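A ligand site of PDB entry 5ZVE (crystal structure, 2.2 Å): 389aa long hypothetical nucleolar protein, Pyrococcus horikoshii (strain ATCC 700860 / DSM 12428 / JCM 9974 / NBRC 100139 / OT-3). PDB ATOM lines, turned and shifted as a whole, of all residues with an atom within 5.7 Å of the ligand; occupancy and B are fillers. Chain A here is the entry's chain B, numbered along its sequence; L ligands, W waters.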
ATOM      1  N   TYR A 180      26.225  37.935 -19.612  1.00  0.00           N
ATOM      2  CA  TYR A 180      25.290  37.301 -18.694  1.00  0.00           C
ATOM      3  C   TYR A 180      25.806  37.434 -17.267  1.00  0.00           C
ATOM      4  O   TYR A 180      26.858  36.900 -16.931  1.00  0.00           O
ATOM      5  CB  TYR A 180      25.091  35.828 -19.068  1.00  0.00           C
ATOM      6  CG  TYR A 180      24.037  35.122 -18.241  1.00  0.00           C
ATOM      7  CD1 TYR A 180      22.704  35.155 -18.623  1.00  0.00           C
ATOM      8  CD2 TYR A 180      24.386  34.433 -17.089  1.00  0.00           C
ATOM      9  CE1 TYR A 180      21.743  34.522 -17.873  1.00  0.00           C
ATOM     10  CE2 TYR A 180      23.425  33.800 -16.339  1.00  0.00           C
ATOM     11  CZ  TYR A 180      22.109  33.842 -16.732  1.00  0.00           C
ATOM     12  OH  TYR A 180      21.144  33.200 -15.986  1.00  0.00           O
ATOM     13  N   GLN A 182      26.681  36.739 -13.680  1.00  0.00           N
ATOM     14  CA  GLN A 182      26.979  35.423 -13.133  1.00  0.00           C
ATOM     15  C   GLN A 182      28.170  35.525 -12.195  1.00  0.00           C
ATOM     16  O   GLN A 182      29.141  36.217 -12.512  1.00  0.00           O
ATOM     17  CB  GLN A 182      27.259  34.427 -14.255  1.00  0.00           C
ATOM     18  CG  GLN A 182      27.396  32.981 -13.810  1.00  0.00           C
ATOM     19  CD  GLN A 182      27.688  32.028 -14.961  1.00  0.00           C
ATOM     20  OE1 GLN A 182      28.442  32.359 -15.886  1.00  0.00           O
ATOM     21  NE2 GLN A 182      27.081  30.846 -14.912  1.00  0.00           N
ATOM     22  N   ASP A 203      23.298  18.872 -18.216  1.00  0.00           N
ATOM     23  CA  ASP A 203      23.053  19.785 -17.105  1.00  0.00           C
ATOM     24  C   ASP A 203      21.690  19.432 -16.521  1.00  0.00           C
ATOM     25  O   ASP A 203      20.662  19.725 -17.122  1.00  0.00           O
ATOM     26  CB  ASP A 203      23.102  21.238 -17.600  1.00  0.00           C
ATOM     27  CG  ASP A 203      23.221  22.245 -16.464  1.00  0.00           C
ATOM     28  OD1 ASP A 203      23.015  21.875 -15.293  1.00  0.00           O
ATOM     29  OD2 ASP A 203      23.545  23.414 -16.757  1.00  0.00           O
ATOM     30  N   MET A 204      21.669  18.791 -15.357  1.00  0.00           N
ATOM     31  CA  MET A 204      20.432  18.178 -14.883  1.00  0.00           C
ATOM     32  C   MET A 204      19.611  19.074 -13.966  1.00  0.00           C
ATOM     33  O   MET A 204      18.520  18.699 -13.545  1.00  0.00           O
ATOM     34  CB  MET A 204      20.709  16.854 -14.155  1.00  0.00           C
ATOM     35  CG  MET A 204      21.803  16.894 -13.106  1.00  0.00           C
ATOM     36  SD  MET A 204      22.016  15.256 -12.350  1.00  0.00           S
ATOM     37  CE  MET A 204      22.487  14.323 -13.768  1.00  0.00           C
ATOM     38  N   ALA A 205      20.129  20.255 -13.669  1.00  0.00           N
ATOM     39  CA  ALA A 205      19.354  21.288 -12.985  1.00  0.00           C
ATOM     40  C   ALA A 205      19.791  22.613 -13.573  1.00  0.00           C
ATOM     41  O   ALA A 205      20.538  23.359 -12.946  1.00  0.00           O
ATOM     42  CB  ALA A 205      19.574  21.245 -11.489  1.00  0.00           C
ATOM     43  N   ALA A 206      19.294  22.906 -14.772  1.00  0.00           N
ATOM     44  CA  ALA A 206      19.974  23.853 -15.650  1.00  0.00           C
ATOM     45  C   ALA A 206      19.399  25.259 -15.668  1.00  0.00           C
ATOM     46  O   ALA A 206      20.129  26.212 -15.921  1.00  0.00           O
ATOM     47  CB  ALA A 206      19.985  23.297 -17.070  1.00  0.00           C
ATOM     48  N   ALA A 207      18.104  25.402 -15.380  1.00  0.00           N
ATOM     49  CA  ALA A 207      17.451  26.708 -15.494  1.00  0.00           C
ATOM     50  C   ALA A 207      17.846  27.636 -14.360  1.00  0.00           C
ATOM     51  O   ALA A 207      18.045  27.183 -13.238  1.00  0.00           O
ATOM     52  CB  ALA A 207      15.941  26.540 -15.547  1.00  0.00           C
ATOM     53  N   PRO A 208      17.955  28.955 -14.636  1.00  0.00           N
ATOM     54  CA  PRO A 208      17.653  29.637 -15.906  1.00  0.00           C
ATOM     55  C   PRO A 208      18.718  29.524 -17.012  1.00  0.00           C
ATOM     56  O   PRO A 208      18.553  30.131 -18.061  1.00  0.00           O
ATOM     57  CB  PRO A 208      17.512  31.098 -15.469  1.00  0.00           C
ATOM     58  CG  PRO A 208      18.425  31.220 -14.308  1.00  0.00           C
ATOM     59  CD  PRO A 208      18.320  29.918 -13.579  1.00  0.00           C
ATOM     60  N   GLY A 209      19.778  28.760 -16.781  1.00  0.00           N
ATOM     61  CA  GLY A 209      20.713  28.454 -17.847  1.00  0.00           C
ATOM     62  C   GLY A 209      22.032  29.201 -17.809  1.00  0.00           C
ATOM     63  O   GLY A 209      22.727  29.299 -18.818  1.00  0.00           O
ATOM     64  N   GLY A 210      22.368  29.724 -16.633  1.00  0.00           N
ATOM     65  CA  GLY A 210      23.646  30.397 -16.435  1.00  0.00           C
ATOM     66  C   GLY A 210      24.834  29.526 -16.810  1.00  0.00           C
ATOM     67  O   GLY A 210      25.649  29.902 -17.655  1.00  0.00           O
ATOM     68  N   LYS A 211      24.920  28.353 -16.203  1.00  0.00           N
ATOM     69  CA  LYS A 211      26.047  27.472 -16.460  1.00  0.00           C
ATOM     70  C   LYS A 211      25.873  26.735 -17.781  1.00  0.00           C
ATOM     71  O   LYS A 211      26.857  26.378 -18.422  1.00  0.00           O
ATOM     72  CB  LYS A 211      26.239  26.478 -15.307  1.00  0.00           C
ATOM     73  CG  LYS A 211      26.646  27.148 -13.998  1.00  0.00           C
ATOM     74  CD  LYS A 211      26.621  26.166 -12.833  1.00  0.00           C
ATOM     75  CE  LYS A 211      27.046  26.851 -11.549  1.00  0.00           C
ATOM     76  NZ  LYS A 211      26.023  27.836 -11.094  1.00  0.00           N
ATOM     77  N   THR A 212      24.636  26.507 -18.181  1.00  0.00           N
ATOM     78  CA  THR A 212      24.403  25.837 -19.458  1.00  0.00           C
ATOM     79  C   THR A 212      24.922  26.657 -20.637  1.00  0.00           C
ATOM     80  O   THR A 212      25.622  26.142 -21.515  1.00  0.00           O
ATOM     81  CB  THR A 212      22.918  25.528 -19.678  1.00  0.00           C
ATOM     82  OG1 THR A 212      22.423  24.746 -18.583  1.00  0.00           O
ATOM     83  CG2 THR A 212      22.726  24.754 -20.977  1.00  0.00           C
ATOM     84  N   ILE A 228      18.293  19.972 -18.299  1.00  0.00           N
ATOM     85  CA  ILE A 228      17.110  19.464 -17.603  1.00  0.00           C
ATOM     86  C   ILE A 228      16.657  20.423 -16.512  1.00  0.00           C
ATOM     87  O   ILE A 228      17.472  20.964 -15.781  1.00  0.00           O
ATOM     88  CB  ILE A 228      17.383  18.090 -16.974  1.00  0.00           C
ATOM     89  CG1 ILE A 228      17.847  17.092 -18.043  1.00  0.00           C
ATOM     90  CG2 ILE A 228      16.178  17.578 -16.219  1.00  0.00           C
ATOM     91  CD1 ILE A 228      18.313  15.788 -17.482  1.00  0.00           C
ATOM     92  N   ASP A 229      15.342  20.626 -16.399  1.00  0.00           N
ATOM     93  CA  ASP A 229      14.781  21.298 -15.238  1.00  0.00           C
ATOM     94  C   ASP A 229      13.326  20.897 -15.052  1.00  0.00           C
ATOM     95  O   ASP A 229      12.636  20.574 -16.013  1.00  0.00           O
ATOM     96  CB  ASP A 229      14.885  22.817 -15.367  1.00  0.00           C
ATOM     97  CG  ASP A 229      14.966  23.504 -14.022  1.00  0.00           C
ATOM     98  OD1 ASP A 229      13.911  23.675 -13.368  1.00  0.00           O
ATOM     99  OD2 ASP A 229      16.085  23.872 -13.601  1.00  0.00           O
ATOM    100  N   LYS A 230      12.866  20.909 -13.810  1.00  0.00           N
ATOM    101  CA  LYS A 230      11.492  20.524 -13.501  1.00  0.00           C
ATOM    102  C   LYS A 230      10.515  21.680 -13.688  1.00  0.00           C
ATOM    103  O   LYS A 230       9.341  21.471 -13.980  1.00  0.00           O
ATOM    104  CB  LYS A 230      11.390  20.014 -12.059  1.00  0.00           C
ATOM    105  CG  LYS A 230      10.077  19.346 -11.732  1.00  0.00           C
ATOM    106  CD  LYS A 230       9.980  18.972 -10.255  1.00  0.00           C
ATOM    107  CE  LYS A 230       9.997  20.216  -9.371  1.00  0.00           C
ATOM    108  NZ  LYS A 230       9.729  19.892  -7.935  1.00  0.00           N
ATOM    109  N   SER A 231      11.021  22.903 -13.558  1.00  0.00           N
ATOM    110  CA  SER A 231      10.160  24.093 -13.592  1.00  0.00           C
ATOM    111  C   SER A 231       9.957  24.584 -15.020  1.00  0.00           C
ATOM    112  O   SER A 231      10.925  24.898 -15.722  1.00  0.00           O
ATOM    113  CB  SER A 231      10.760  25.206 -12.724  1.00  0.00           C
ATOM    114  OG  SER A 231       9.910  26.330 -12.671  1.00  0.00           O
ATOM    115  N   ARG A 234      10.839  28.517 -15.172  1.00  0.00           N
ATOM    116  CA  ARG A 234      12.279  28.719 -15.205  1.00  0.00           C
ATOM    117  C   ARG A 234      12.871  28.234 -16.532  1.00  0.00           C
ATOM    118  O   ARG A 234      13.837  28.798 -17.043  1.00  0.00           O
ATOM    119  CB  ARG A 234      12.950  28.030 -14.013  1.00  0.00           C
ATOM    120  CG  ARG A 234      12.543  28.647 -12.668  1.00  0.00           C
ATOM    121  CD  ARG A 234      13.036  27.822 -11.489  1.00  0.00           C
ATOM    122  NE  ARG A 234      14.493  27.791 -11.383  1.00  0.00           N
ATOM    123  CZ  ARG A 234      15.254  28.790 -10.948  1.00  0.00           C
ATOM    124  NH1 ARG A 234      14.702  29.933 -10.570  1.00  0.00           N
ATOM    125  NH2 ARG A 234      16.572  28.645 -10.898  1.00  0.00           N
ATOM    126  N   MET A 255      11.591  17.647 -16.909  1.00  0.00           N
ATOM    127  CA  MET A 255      11.467  16.367 -16.210  1.00  0.00           C
ATOM    128  C   MET A 255      12.062  16.439 -14.809  1.00  0.00           C
ATOM    129  O   MET A 255      12.841  17.339 -14.493  1.00  0.00           O
ATOM    130  CB  MET A 255      12.154  15.247 -16.984  1.00  0.00           C
ATOM    131  CG  MET A 255      13.656  15.220 -16.799  1.00  0.00           C
ATOM    132  SD  MET A 255      14.482  13.850 -17.634  1.00  0.00           S
ATOM    133  CE  MET A 255      13.933  12.463 -16.643  1.00  0.00           C
ATOM    134  N   ASP A 256      11.691  15.472 -13.969  1.00  0.00           N
ATOM    135  CA  ASP A 256      12.328  15.263 -12.673  1.00  0.00           C
ATOM    136  C   ASP A 256      13.693  14.631 -12.915  1.00  0.00           C
ATOM    137  O   ASP A 256      13.789  13.482 -13.343  1.00  0.00           O
ATOM    138  CB  ASP A 256      11.460  14.391 -11.771  1.00  0.00           C
ATOM    139  CG  ASP A 256      12.082  14.137 -10.409  1.00  0.00           C
ATOM    140  OD1 ASP A 256      13.156  14.698 -10.114  1.00  0.00           O
ATOM    141  OD2 ASP A 256      11.497  13.354  -9.630  1.00  0.00           O
ATOM    142  N   ALA A 257      14.758  15.391 -12.635  1.00  0.00           N
ATOM    143  CA  ALA A 257      16.122  14.957 -12.924  1.00  0.00           C
ATOM    144  C   ALA A 257      16.539  13.709 -12.140  1.00  0.00           C
ATOM    145  O   ALA A 257      17.494  13.027 -12.512  1.00  0.00           O
ATOM    146  CB  ALA A 257      17.104  16.077 -12.652  1.00  0.00           C
ATOM    147  N   ARG A 258      15.825  13.435 -11.059  1.00  0.00           N
ATOM    148  CA  ARG A 258      16.100  12.260 -10.237  1.00  0.00           C
ATOM    149  C   ARG A 258      15.780  10.969 -10.987  1.00  0.00           C
ATOM    150  O   ARG A 258      16.258   9.896 -10.621  1.00  0.00           O
ATOM    151  CB  ARG A 258      15.310  12.328  -8.935  1.00  0.00           C
ATOM    152  CG  ARG A 258      15.771  13.430  -8.003  1.00  0.00           C
ATOM    153  CD  ARG A 258      14.811  13.613  -6.844  1.00  0.00           C
ATOM    154  NE  ARG A 258      13.428  13.780  -7.291  1.00  0.00           N
ATOM    155  CZ  ARG A 258      12.395  13.855  -6.463  1.00  0.00           C
ATOM    156  NH1 ARG A 258      11.171  14.016  -6.959  1.00  0.00           N
ATOM    157  NH2 ARG A 258      12.582  13.766  -5.156  1.00  0.00           N
ATOM    158  N   LEU A 271      26.972  18.028 -15.337  1.00  0.00           N
ATOM    159  CA  LEU A 271      26.974  19.100 -14.365  1.00  0.00           C
ATOM    160  C   LEU A 271      25.766  19.003 -13.442  1.00  0.00           C
ATOM    161  O   LEU A 271      24.627  18.931 -13.898  1.00  0.00           O
ATOM    162  CB  LEU A 271      26.980  20.468 -15.058  1.00  0.00           C
ATOM    163  CG  LEU A 271      26.757  21.635 -14.093  1.00  0.00           C
ATOM    164  CD1 LEU A 271      27.888  21.712 -13.089  1.00  0.00           C
ATOM    165  CD2 LEU A 271      26.625  22.954 -14.854  1.00  0.00           C
ATOM    166  N   ASP A 273      24.491  21.338 -10.760  1.00  0.00           N
ATOM    167  CA  ASP A 273      24.431  22.569  -9.983  1.00  0.00           C
ATOM    168  C   ASP A 273      23.148  22.485  -9.176  1.00  0.00           C
ATOM    169  O   ASP A 273      22.106  22.991  -9.571  1.00  0.00           O
ATOM    170  CB  ASP A 273      24.457  23.787 -10.901  1.00  0.00           C
ATOM    171  CG  ASP A 273      24.495  25.093 -10.129  1.00  0.00           C
ATOM    172  OD1 ASP A 273      25.148  25.140  -9.062  1.00  0.00           O
ATOM    173  OD2 ASP A 273      23.869  26.067 -10.600  1.00  0.00           O
ATOM    174  N   ALA A 274      23.237  21.850  -8.009  1.00  0.00           N
ATOM    175  CA  ALA A 274      22.079  21.269  -7.361  1.00  0.00           C
ATOM    176  C   ALA A 274      21.252  22.289  -6.590  1.00  0.00           C
ATOM    177  O   ALA A 274      21.796  23.255  -6.039  1.00  0.00           O
ATOM    178  CB  ALA A 274      22.509  20.152  -6.428  1.00  0.00           C
ATOM    179  N   PRO A 275      19.922  22.094  -6.554  1.00  0.00           N
ATOM    180  CA  PRO A 275      19.066  22.839  -5.632  1.00  0.00           C
ATOM    181  C   PRO A 275      19.606  22.684  -4.221  1.00  0.00           C
ATOM    182  O   PRO A 275      19.975  21.579  -3.829  1.00  0.00           O
ATOM    183  CB  PRO A 275      17.696  22.174  -5.804  1.00  0.00           C
ATOM    184  CG  PRO A 275      17.974  20.856  -6.449  1.00  0.00           C
ATOM    185  CD  PRO A 275      19.157  21.087  -7.323  1.00  0.00           C
ATOM    186  N   TYR A 300      17.745  15.225  -0.316  1.00  0.00           N
ATOM    187  CA  TYR A 300      17.129  15.452  -1.620  1.00  0.00           C
ATOM    188  C   TYR A 300      18.173  15.449  -2.740  1.00  0.00           C
ATOM    189  O   TYR A 300      17.921  14.945  -3.832  1.00  0.00           O
ATOM    190  CB  TYR A 300      16.364  16.784  -1.593  1.00  0.00           C
ATOM    191  CG  TYR A 300      15.654  17.172  -2.867  1.00  0.00           C
ATOM    192  CD1 TYR A 300      14.664  16.361  -3.414  1.00  0.00           C
ATOM    193  CD2 TYR A 300      15.949  18.375  -3.514  1.00  0.00           C
ATOM    194  CE1 TYR A 300      14.002  16.723  -4.569  1.00  0.00           C
ATOM    195  CE2 TYR A 300      15.287  18.736  -4.669  1.00  0.00           C
ATOM    196  CZ  TYR A 300      14.316  17.910  -5.200  1.00  0.00           C
ATOM    197  OH  TYR A 300      13.654  18.271  -6.355  1.00  0.00           O
ATOM    198  N   PHE A 304      19.580  13.087  -6.855  1.00  0.00           N
ATOM    199  CA  PHE A 304      20.201  13.616  -8.073  1.00  0.00           C
ATOM    200  C   PHE A 304      21.554  12.970  -8.352  1.00  0.00           C
ATOM    201  O   PHE A 304      21.842  12.522  -9.464  1.00  0.00           O
ATOM    202  CB  PHE A 304      20.393  15.130  -7.981  1.00  0.00           C
ATOM    203  CG  PHE A 304      19.123  15.917  -7.957  1.00  0.00           C
ATOM    204  CD1 PHE A 304      18.343  15.979  -6.818  1.00  0.00           C
ATOM    205  CD2 PHE A 304      18.726  16.646  -9.069  1.00  0.00           C
ATOM    206  CE1 PHE A 304      17.170  16.720  -6.790  1.00  0.00           C
ATOM    207  CE2 PHE A 304      17.553  17.392  -9.055  1.00  0.00           C
ATOM    208  CZ  PHE A 304      16.782  17.435  -7.909  1.00  0.00           C
HETATM  209  N1  LIG L   1      22.309  25.776 -12.773  1.00  0.00           N
HETATM  210  C1  LIG L   1      21.399  26.907 -12.916  1.00  0.00           C
HETATM  211  C2  LIG L   1      20.669  27.204 -11.608  1.00  0.00           C
HETATM  212  C3  LIG L   1      20.220  25.987 -10.790  1.00  0.00           C
HETATM  213  S1  LIG L   1      19.032  26.461  -9.516  1.00  0.00           S
HETATM  214  C4  LIG L   1      22.093  28.163 -13.455  1.00  0.00           C
HETATM  215  O1  LIG L   1      23.317  28.265 -13.493  1.00  0.00           O
HETATM  216  O2  LIG L   1      21.437  29.116 -13.874  1.00  0.00           O
HETATM  217  C5  LIG L   1      18.450  24.762  -9.249  1.00  0.00           C
HETATM  218  C6  LIG L   1      17.384  24.293 -10.236  1.00  0.00           C
HETATM  219  O3  LIG L   1      17.023  22.956  -9.953  1.00  0.00           O
HETATM  220  C7  LIG L   1      16.091  25.093 -10.191  1.00  0.00           C
HETATM  221  O4  LIG L   1      15.908  25.752 -11.425  1.00  0.00           O
HETATM  222  C8  LIG L   1      14.978  24.079 -10.018  1.00  0.00           C
HETATM  223  O5  LIG L   1      13.965  24.300 -10.965  1.00  0.00           O
HETATM  224  C9  LIG L   1      15.675  22.769 -10.328  1.00  0.00           C
HETATM  225  N2  LIG L   1      15.088  21.594  -9.654  1.00  0.00           N
HETATM  226  C10 LIG L   1      14.649  21.480  -8.359  1.00  0.00           C
HETATM  227  N3  LIG L   1      14.187  20.215  -8.162  1.00  0.00           N
HETATM  228  C11 LIG L   1      14.326  19.522  -9.317  1.00  0.00           C
HETATM  229  C12 LIG L   1      14.021  18.220  -9.672  1.00  0.00           C
HETATM  230  N4  LIG L   1      13.480  17.377  -8.803  1.00  0.00           N
HETATM  231  N5  LIG L   1      14.286  17.787 -10.963  1.00  0.00           N
HETATM  232  C13 LIG L   1      14.847  18.664 -11.879  1.00  0.00           C
HETATM  233  N6  LIG L   1      15.142  19.957 -11.520  1.00  0.00           N
HETATM  234  C14 LIG L   1      14.893  20.382 -10.256  1.00  0.00           C
HETATM  235  O   HOH W   1      22.628  25.841 -15.811  1.00  0.00           O
HETATM  236  O   HOH W   2      25.115  30.353 -12.607  1.00  0.00           O
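Ala 206 touches the ligand. CD of Pro 208 touches O2 of the ligand, 3.2 Å away. Ser 231 touches the ligand. Met 255 touches the ligand. Arg 258 touches the ligand (NE to N4, 3.9 Å). Pro 275 touches the ligand (CD to O3, 3.9 Å). Phe 304 touches the ligand (CZ to C12, 3.4 Å). Within 4 Å of the ligand: Ala 205, Ala 206, Ala 207, Pro 208, Gly 209, Gly 210, Lys 211, Asp 229, Lys 230, Ser 231, Arg 234, Met 255, Asp 256, Ala 257, Arg 258, Asp 273, Pro 275, Tyr 300 and Phe 304. The nearest printed residue that does not touch the ligand is Met 204 (4.03 Å).
A nitrogen (N5) of the ligand is in hydrogen-bond range of the backbone NH (N) of Ala 257, 3.0 Å away. An oxygen (O4) of the ligand is in hydrogen-bond range of the guanidinium group of Arg 234 (2.5 Å). An oxygen (O4) of the ligand sits close to the backbone carbonyl oxygen of Ala 207 (3.1 Å). A nitrogen (N4) of the ligand sits at hydrogen-bond distance from the side-chain carboxylate of Asp 256, 3.0 Å away. The backbone NH (N) of Lys 211 is in hydrogen-bond range of an oxygen (O1) of the ligand (3.1 Å). The side-chain hydroxyl of Tyr 300 sits at hydrogen-bond distance from a nitrogen (N4) of the ligand, at 2.6 Å. N1 of the ligand lies within hydrogen-bond range of O of Ala 205 (3.0 Å). O2 of the ligand lies within hydrogen-bond range of N of Gly 209 (3.4 Å). The side-chain carboxylate (OD2) of Asp 273 lies within salt-bridge range of a nitrogen (N1) of the ligand (2.7 Å). The side-chain carboxylate (OD1) of Asp 229 sits at hydrogen-bond distance from an oxygen (O5) of the ligand (2.5 Å). The backbone NH (N) of Gly 210 is in hydrogen-bond range of an oxygen (O2) of the ligand (3.0 Å). N of Lys 230 sits at hydrogen-bond distance from N6 of the ligand, 3.4 Å away. NZ of Lys 211 is in salt-bridge range of O1 of the ligand (3.6 Å).
Water W2 lies within hydrogen-bond range of O1 of the ligand (2.9 Å), NE2 of Gln 182 (3.1 Å) and NZ of Lys 211 (3.1 Å). Water W1 lies within hydrogen-bond range of O of Ala 206 (2.5 Å), OD2 of Asp 203 (2.8 Å), OG1 of Thr 212 (3.0 Å), N1 of the ligand (3.1 Å) and N of Lys 211 (3.4 Å).
O of Gly 210 lies close to NE2 of Gln 182, at 3.2 Å. N of Ala 205 lies close to O of Ile 228 (3.5 Å). O of Asp 229 sits at hydrogen-bond distance from N of Met 255 (3.2 Å). The backbone NH (N) of Arg 234 is in hydrogen-bond range of the side-chain hydroxyl (OG) of Ser 231 (3.4 Å). O of Ile 228 lies within hydrogen-bond range of N of Ala 206 (2.8 Å). The backbone NH of Ala 207 is in hydrogen-bond range of the side-chain carboxylate of Asp 229 (3.1 Å). OD1 of Asp 229 is in hydrogen-bond range of N of Ser 231, at 3.0 Å. The guanidinium group of Arg 234 is in hydrogen-bond range of the backbone carbonyl oxygen of Ala 207, 3.1 Å away.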
